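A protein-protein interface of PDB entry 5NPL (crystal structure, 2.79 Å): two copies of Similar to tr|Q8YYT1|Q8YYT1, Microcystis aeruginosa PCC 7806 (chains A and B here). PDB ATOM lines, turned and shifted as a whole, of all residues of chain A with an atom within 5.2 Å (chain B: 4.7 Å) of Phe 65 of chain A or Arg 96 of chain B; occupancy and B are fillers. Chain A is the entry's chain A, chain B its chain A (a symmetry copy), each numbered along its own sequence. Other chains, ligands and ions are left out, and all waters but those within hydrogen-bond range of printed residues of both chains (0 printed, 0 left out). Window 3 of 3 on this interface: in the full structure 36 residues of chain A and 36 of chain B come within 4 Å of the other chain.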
ATOM      1  N   TYR A  60     -23.215  -0.611  26.643  1.00  0.00           N
ATOM      2  CA  TYR A  60     -23.452  -1.843  25.876  1.00  0.00           C
ATOM      3  C   TYR A  60     -24.317  -1.616  24.636  1.00  0.00           C
ATOM      4  O   TYR A  60     -24.053  -2.191  23.599  1.00  0.00           O
ATOM      5  CB  TYR A  60     -24.108  -2.911  26.746  1.00  0.00           C
ATOM      6  CG  TYR A  60     -23.238  -3.604  27.794  1.00  0.00           C
ATOM      7  CD1 TYR A  60     -21.952  -3.142  28.161  1.00  0.00           C
ATOM      8  CD2 TYR A  60     -23.721  -4.707  28.447  1.00  0.00           C
ATOM      9  CE1 TYR A  60     -21.199  -3.782  29.130  1.00  0.00           C
ATOM     10  CE2 TYR A  60     -22.978  -5.364  29.408  1.00  0.00           C
ATOM     11  CZ  TYR A  60     -21.714  -4.902  29.750  1.00  0.00           C
ATOM     12  OH  TYR A  60     -21.028  -5.609  30.698  1.00  0.00           O
ATOM     13  N   LYS A  61     -25.345  -0.786  24.722  1.00  0.00           N
ATOM     14  CA  LYS A  61     -26.270  -0.629  23.586  1.00  0.00           C
ATOM     15  C   LYS A  61     -25.987   0.513  22.621  1.00  0.00           C
ATOM     16  O   LYS A  61     -26.506   0.480  21.527  1.00  0.00           O
ATOM     17  CB  LYS A  61     -27.695  -0.514  24.081  1.00  0.00           C
ATOM     18  CG  LYS A  61     -28.086  -1.740  24.875  1.00  0.00           C
ATOM     19  CD  LYS A  61     -29.437  -1.586  25.536  1.00  0.00           C
ATOM     20  CE  LYS A  61     -29.603  -2.623  26.632  1.00  0.00           C
ATOM     21  NZ  LYS A  61     -30.985  -2.578  27.155  1.00  0.00           N
ATOM     22  N   VAL A  62     -25.182   1.491  23.009  1.00  0.00           N
ATOM     23  CA  VAL A  62     -24.916   2.648  22.167  1.00  0.00           C
ATOM     24  C   VAL A  62     -23.433   2.777  21.852  1.00  0.00           C
ATOM     25  O   VAL A  62     -23.071   2.778  20.681  1.00  0.00           O
ATOM     26  CB  VAL A  62     -25.450   3.945  22.840  1.00  0.00           C
ATOM     27  CG1 VAL A  62     -25.260   5.160  21.967  1.00  0.00           C
ATOM     28  CG2 VAL A  62     -26.915   3.778  23.178  1.00  0.00           C
ATOM     29  N   ALA A  63     -22.591   2.924  22.874  1.00  0.00           N
ATOM     30  CA  ALA A  63     -21.110   3.064  22.690  1.00  0.00           C
ATOM     31  C   ALA A  63     -20.456   1.885  21.968  1.00  0.00           C
ATOM     32  O   ALA A  63     -19.672   2.078  21.040  1.00  0.00           O
ATOM     33  CB  ALA A  63     -20.405   3.299  24.021  1.00  0.00           C
ATOM     34  N   ALA A  64     -20.816   0.676  22.372  1.00  0.00           N
ATOM     35  CA  ALA A  64     -20.227  -0.568  21.822  1.00  0.00           C
ATOM     36  C   ALA A  64     -20.562  -0.838  20.352  1.00  0.00           C
ATOM     37  O   ALA A  64     -19.894  -1.664  19.738  1.00  0.00           O
ATOM     38  CB  ALA A  64     -20.667  -1.768  22.654  1.00  0.00           C
ATOM     39  N   PHE A  65     -21.614  -0.201  19.819  1.00  0.00           N
ATOM     40  CA  PHE A  65     -21.940  -0.252  18.397  1.00  0.00           C
ATOM     41  C   PHE A  65     -21.545   0.978  17.645  1.00  0.00           C
ATOM     42  O   PHE A  65     -21.485   0.940  16.421  1.00  0.00           O
ATOM     43  CB  PHE A  65     -23.422  -0.507  18.214  1.00  0.00           C
ATOM     44  CG  PHE A  65     -23.827  -1.833  18.744  1.00  0.00           C
ATOM     45  CD1 PHE A  65     -23.686  -2.968  17.959  1.00  0.00           C
ATOM     46  CD2 PHE A  65     -24.254  -1.980  20.055  1.00  0.00           C
ATOM     47  CE1 PHE A  65     -24.011  -4.213  18.464  1.00  0.00           C
ATOM     48  CE2 PHE A  65     -24.566  -3.225  20.569  1.00  0.00           C
ATOM     49  CZ  PHE A  65     -24.451  -4.342  19.769  1.00  0.00           C
ATOM     50  N   GLY A  66     -21.262   2.066  18.363  1.00  0.00           N
ATOM     51  CA  GLY A  66     -20.981   3.343  17.738  1.00  0.00           C
ATOM     52  C   GLY A  66     -22.226   4.058  17.239  1.00  0.00           C
ATOM     53  O   GLY A  66     -22.121   4.882  16.329  1.00  0.00           O
ATOM     54  N   HIS A  67     -23.379   3.788  17.860  1.00  0.00           N
ATOM     55  CA  HIS A  67     -24.584   4.566  17.559  1.00  0.00           C
ATOM     56  C   HIS A  67     -24.460   6.005  17.995  1.00  0.00           C
ATOM     57  O   HIS A  67     -23.661   6.309  18.882  1.00  0.00           O
ATOM     58  CB  HIS A  67     -25.847   3.940  18.155  1.00  0.00           C
ATOM     59  CG  HIS A  67     -26.163   2.601  17.574  1.00  0.00           C
ATOM     60  ND1 HIS A  67     -26.627   1.555  18.337  1.00  0.00           N
ATOM     61  CD2 HIS A  67     -26.028   2.118  16.313  1.00  0.00           C
ATOM     62  CE1 HIS A  67     -26.781   0.485  17.576  1.00  0.00           C
ATOM     63  NE2 HIS A  67     -26.417   0.799  16.346  1.00  0.00           N
ATOM     64  N   GLU B  92     -14.233   2.933  22.104  1.00  0.00           N
ATOM     65  CA  GLU B  92     -15.348   2.250  21.462  1.00  0.00           C
ATOM     66  C   GLU B  92     -15.105   0.746  21.455  1.00  0.00           C
ATOM     67  O   GLU B  92     -16.025  -0.034  21.607  1.00  0.00           O
ATOM     68  CB  GLU B  92     -15.624   2.827  20.059  1.00  0.00           C
ATOM     69  CG  GLU B  92     -14.725   2.353  18.895  1.00  0.00           C
ATOM     70  CD  GLU B  92     -13.457   3.192  18.690  1.00  0.00           C
ATOM     71  OE1 GLU B  92     -12.945   3.773  19.672  1.00  0.00           O
ATOM     72  OE2 GLU B  92     -12.989   3.275  17.525  1.00  0.00           O
ATOM     73  N   TYR B  93     -13.840   0.346  21.314  1.00  0.00           N
ATOM     74  CA  TYR B  93     -13.436  -1.052  21.464  1.00  0.00           C
ATOM     75  C   TYR B  93     -13.523  -1.519  22.905  1.00  0.00           C
ATOM     76  O   TYR B  93     -13.948  -2.643  23.132  1.00  0.00           O
ATOM     77  CB  TYR B  93     -12.068  -1.315  20.876  1.00  0.00           C
ATOM     78  CG  TYR B  93     -12.053  -1.177  19.387  1.00  0.00           C
ATOM     79  CD1 TYR B  93     -12.797  -2.007  18.582  1.00  0.00           C
ATOM     80  CD2 TYR B  93     -11.296  -0.185  18.779  1.00  0.00           C
ATOM     81  CE1 TYR B  93     -12.764  -1.870  17.206  1.00  0.00           C
ATOM     82  CE2 TYR B  93     -11.280  -0.026  17.386  1.00  0.00           C
ATOM     83  CZ  TYR B  93     -12.005  -0.890  16.611  1.00  0.00           C
ATOM     84  OH  TYR B  93     -11.974  -0.763  15.242  1.00  0.00           O
ATOM     85  N   VAL B  94     -13.175  -0.680  23.875  1.00  0.00           N
ATOM     86  CA  VAL B  94     -13.339  -1.076  25.274  1.00  0.00           C
ATOM     87  C   VAL B  94     -14.806  -1.340  25.579  1.00  0.00           C
ATOM     88  O   VAL B  94     -15.162  -2.351  26.191  1.00  0.00           O
ATOM     89  CB  VAL B  94     -12.850  -0.033  26.272  1.00  0.00           C
ATOM     90  CG1 VAL B  94     -13.049  -0.605  27.699  1.00  0.00           C
ATOM     91  CG2 VAL B  94     -11.391   0.305  26.047  1.00  0.00           C
ATOM     92  N   ALA B  95     -15.644  -0.403  25.156  1.00  0.00           N
ATOM     93  CA  ALA B  95     -17.116  -0.528  25.245  1.00  0.00           C
ATOM     94  C   ALA B  95     -17.560  -1.869  24.716  1.00  0.00           C
ATOM     95  O   ALA B  95     -18.340  -2.537  25.355  1.00  0.00           O
ATOM     96  CB  ALA B  95     -17.808   0.603  24.481  1.00  0.00           C
ATOM     97  N   ARG B  96     -17.021  -2.264  23.565  1.00  0.00           N
ATOM     98  CA  ARG B  96     -17.407  -3.514  22.925  1.00  0.00           C
ATOM     99  C   ARG B  96     -16.872  -4.761  23.612  1.00  0.00           C
ATOM    100  O   ARG B  96     -17.614  -5.754  23.743  1.00  0.00           O
ATOM    101  CB  ARG B  96     -16.991  -3.539  21.469  1.00  0.00           C
ATOM    102  CG  ARG B  96     -17.830  -4.547  20.699  1.00  0.00           C
ATOM    103  CD  ARG B  96     -17.453  -4.577  19.252  1.00  0.00           C
ATOM    104  NE  ARG B  96     -18.278  -5.527  18.512  1.00  0.00           N
ATOM    105  CZ  ARG B  96     -19.444  -5.256  17.899  1.00  0.00           C
ATOM    106  NH1 ARG B  96     -20.008  -4.041  17.935  1.00  0.00           N
ATOM    107  NH2 ARG B  96     -20.036  -6.228  17.212  1.00  0.00           N
ATOM    108  N   LEU B  97     -15.591  -4.727  24.016  1.00  0.00           N
ATOM    109  CA  LEU B  97     -14.987  -5.810  24.769  1.00  0.00           C
ATOM    110  C   LEU B  97     -15.866  -6.061  25.987  1.00  0.00           C
ATOM    111  O   LEU B  97     -16.213  -7.211  26.304  1.00  0.00           O
ATOM    112  CB  LEU B  97     -13.547  -5.466  25.179  1.00  0.00           C
ATOM    113  CG  LEU B  97     -12.811  -6.438  26.158  1.00  0.00           C
ATOM    114  CD1 LEU B  97     -12.786  -7.842  25.591  1.00  0.00           C
ATOM    115  CD2 LEU B  97     -11.434  -6.009  26.528  1.00  0.00           C
ATOM    116  N   PHE B  98     -16.244  -4.964  26.648  1.00  0.00           N
ATOM    117  CA  PHE B  98     -17.091  -5.049  27.824  1.00  0.00           C
ATOM    118  C   PHE B  98     -18.456  -5.681  27.498  1.00  0.00           C
ATOM    119  O   PHE B  98     -18.908  -6.549  28.218  1.00  0.00           O
ATOM    120  CB  PHE B  98     -17.235  -3.666  28.478  1.00  0.00           C
ATOM    121  CG  PHE B  98     -16.034  -3.220  29.286  1.00  0.00           C
ATOM    122  CD1 PHE B  98     -14.814  -3.922  29.297  1.00  0.00           C
ATOM    123  CD2 PHE B  98     -16.107  -2.055  30.035  1.00  0.00           C
ATOM    124  CE1 PHE B  98     -13.723  -3.474  30.039  1.00  0.00           C
ATOM    125  CE2 PHE B  98     -15.035  -1.627  30.792  1.00  0.00           C
ATOM    126  CZ  PHE B  98     -13.847  -2.356  30.792  1.00  0.00           C
ATOM    127  N   ALA B  99     -19.095  -5.271  26.414  1.00  0.00           N
ATOM    128  CA  ALA B  99     -20.385  -5.849  26.058  1.00  0.00           C
ATOM    129  C   ALA B  99     -20.265  -7.329  25.725  1.00  0.00           C
ATOM    130  O   ALA B  99     -21.025  -8.133  26.241  1.00  0.00           O
ATOM    131  CB  ALA B  99     -21.018  -5.095  24.888  1.00  0.00           C
ATOM    132  N   GLN B 100     -19.298  -7.687  24.889  1.00  0.00           N
ATOM    133  CA  GLN B 100     -19.107  -9.086  24.505  1.00  0.00           C
ATOM    134  C   GLN B 100     -18.769 -10.038  25.675  1.00  0.00           C
ATOM    135  O   GLN B 100     -19.244 -11.157  25.692  1.00  0.00           O
ATOM    136  CB  GLN B 100     -18.030  -9.203  23.425  1.00  0.00           C
ATOM    137  CG  GLN B 100     -18.571  -9.073  21.996  1.00  0.00           C
ATOM    138  CD  GLN B 100     -17.467  -9.037  20.939  1.00  0.00           C
ATOM    139  OE1 GLN B 100     -17.670  -8.490  19.817  1.00  0.00           O
ATOM    140  NE2 GLN B 100     -16.270  -9.573  21.298  1.00  0.00           N
ATOM    141  N   LYS B 134     -18.712   7.060  15.933  1.00  0.00           N
ATOM    142  CA  LYS B 134     -18.294   6.347  14.736  1.00  0.00           C
ATOM    143  C   LYS B 134     -18.728   4.931  14.875  1.00  0.00           C
ATOM    144  O   LYS B 134     -18.409   4.299  15.895  1.00  0.00           O
ATOM    145  CB  LYS B 134     -16.767   6.385  14.562  1.00  0.00           C
ATOM    146  CG  LYS B 134     -16.292   5.933  13.169  1.00  0.00           C
ATOM    147  CD  LYS B 134     -14.794   5.692  13.106  1.00  0.00           C
ATOM    148  CE  LYS B 134     -14.430   4.351  13.726  1.00  0.00           C
ATOM    149  NZ  LYS B 134     -12.979   4.289  14.070  1.00  0.00           N
ATOM    150  N   ARG B 135     -19.421   4.418  13.866  1.00  0.00           N
ATOM    151  CA  ARG B 135     -19.890   3.028  13.882  1.00  0.00           C
ATOM    152  C   ARG B 135     -18.672   2.081  13.825  1.00  0.00           C
ATOM    153  O   ARG B 135     -17.688   2.389  13.124  1.00  0.00           O
ATOM    154  CB  ARG B 135     -20.907   2.775  12.753  1.00  0.00           C
ATOM    155  CG  ARG B 135     -21.340   1.329  12.614  1.00  0.00           C
ATOM    156  CD  ARG B 135     -22.770   1.166  12.112  1.00  0.00           C
ATOM    157  NE  ARG B 135     -23.142   2.209  11.144  1.00  0.00           N
ATOM    158  CZ  ARG B 135     -22.933   2.138   9.835  1.00  0.00           C
ATOM    159  NH1 ARG B 135     -22.372   1.096   9.280  1.00  0.00           N
ATOM    160  NH2 ARG B 135     -23.301   3.115   9.051  1.00  0.00           N
ATOM    161  N   LEU B 136     -18.717   0.979  14.573  1.00  0.00           N
ATOM    162  CA  LEU B 136     -17.561   0.106  14.641  1.00  0.00           C
ATOM    163  C   LEU B 136     -17.474  -0.642  13.332  1.00  0.00           C
ATOM    164  O   LEU B 136     -18.522  -1.050  12.770  1.00  0.00           O
ATOM    165  CB  LEU B 136     -17.629  -0.904  15.799  1.00  0.00           C
ATOM    166  CG  LEU B 136     -17.198  -0.498  17.206  1.00  0.00           C
ATOM    167  CD1 LEU B 136     -15.706  -0.823  17.366  1.00  0.00           C
ATOM    168  CD2 LEU B 136     -17.625   0.953  17.505  1.00  0.00           C
ATOM    169  N   PHE B 137     -16.229  -0.772  12.826  1.00  0.00           N
ATOM    170  CA  PHE B 137     -15.939  -1.509  11.608  1.00  0.00           C
ATOM    171  C   PHE B 137     -16.527  -0.893  10.358  1.00  0.00           C
ATOM    172  O   PHE B 137     -16.622  -1.581   9.368  1.00  0.00           O
ATOM    173  CB  PHE B 137     -16.392  -2.992  11.712  1.00  0.00           C
ATOM    174  CG  PHE B 137     -16.183  -3.622  13.056  1.00  0.00           C
ATOM    175  CD1 PHE B 137     -14.984  -3.503  13.711  1.00  0.00           C
ATOM    176  CD2 PHE B 137     -17.191  -4.380  13.624  1.00  0.00           C
ATOM    177  CE1 PHE B 137     -14.754  -4.159  14.922  1.00  0.00           C
ATOM    178  CE2 PHE B 137     -17.003  -5.018  14.839  1.00  0.00           C
ATOM    179  CZ  PHE B 137     -15.782  -4.884  15.525  1.00  0.00           C
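Of the printed residues of chain B, Ala 63 of chain A touches Ala 95. Of the printed residues of chain B, Gly 66 of chain A touches Lys 134, Arg 135 and Leu 136. His 67 of chain A touches none of the printed residues of chain B. Of the printed residues of chain A, Ala 95 of chain B touches Ala 63 and Ala 64. Of chain A, only Ala 64 and Phe 65 come within 4 Å of Arg 96 of chain B. Of the printed residues of chain A, Lys 134 of chain B touches Gly 66 (3.3 Å). Of the printed residues of chain A, Leu 136 of chain B touches Ala 64, Phe 65 and Gly 66. The nearest printed residue of chain A that does not touch Leu 136 of chain B is Ala 63 of chain A (4.2 Å).
No position is printed for both chains.
The side-chain carboxylate (OE2) of Glu 92 of chain B is in salt-bridge range of the side-chain amino group (NZ) of Lys 134 of chain B, at 3.6 Å. The side-chain amide oxygen (OE1) of Gln 100 of chain B lies within hydrogen-bond range of the guanidinium group (NE) of Arg 96 of chain B (3.3 Å).
Hydrophobic or aromatic side chains of chain A within 4 Å of the printed part of chain B: Tyr 60, Ala 63, Ala 64 and Phe 65. Hydrophobic or aromatic side chains of chain B that line the printed part of chain A: Ala 95, Ala 99 and Leu 136. Among the printed residues, no Asp or Glu carboxylate lies within 4 Å of a Lys or Arg side-chain nitrogen of the other chain.
O of Ala 64 of chain A sits at hydrogen-bond distance from NH1 of Arg 96 of chain B, 3.0 Å away. OH of Tyr 60 of chain A is in hydrogen-bond range of O of Phe 98 of chain B, 3.4 Å away. The backbone carbonyl oxygen of Phe 65 of chain A sits at hydrogen-bond distance from the backbone NH of Leu 136 of chain B, at 3.3 Å.
Among the printed residues, merely in contact across the chains: Tyr 60 of chain A with Ala 99 of chain B (3.7 Å), Ala 63 of chain A with Ala 95 of chain B (3.8 Å), Ala 64 of chain A with Ala 95 of chain B (3.6 Å), Ala 64 of chain A with Leu 136 of chain B (3.9 Å), Phe 65 of chain A with Arg 96 of chain B (3.8 Å), Phe 65 of chain A with Arg 135 of chain B (3.7 Å), Gly 66 of chain A with Lys 134 of chain B (3.3 Å), Gly 66 of chain A with Arg 135 of chain B (3.7 Å) and Gly 66 of chain A with Leu 136 of chain B (3.9 Å).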
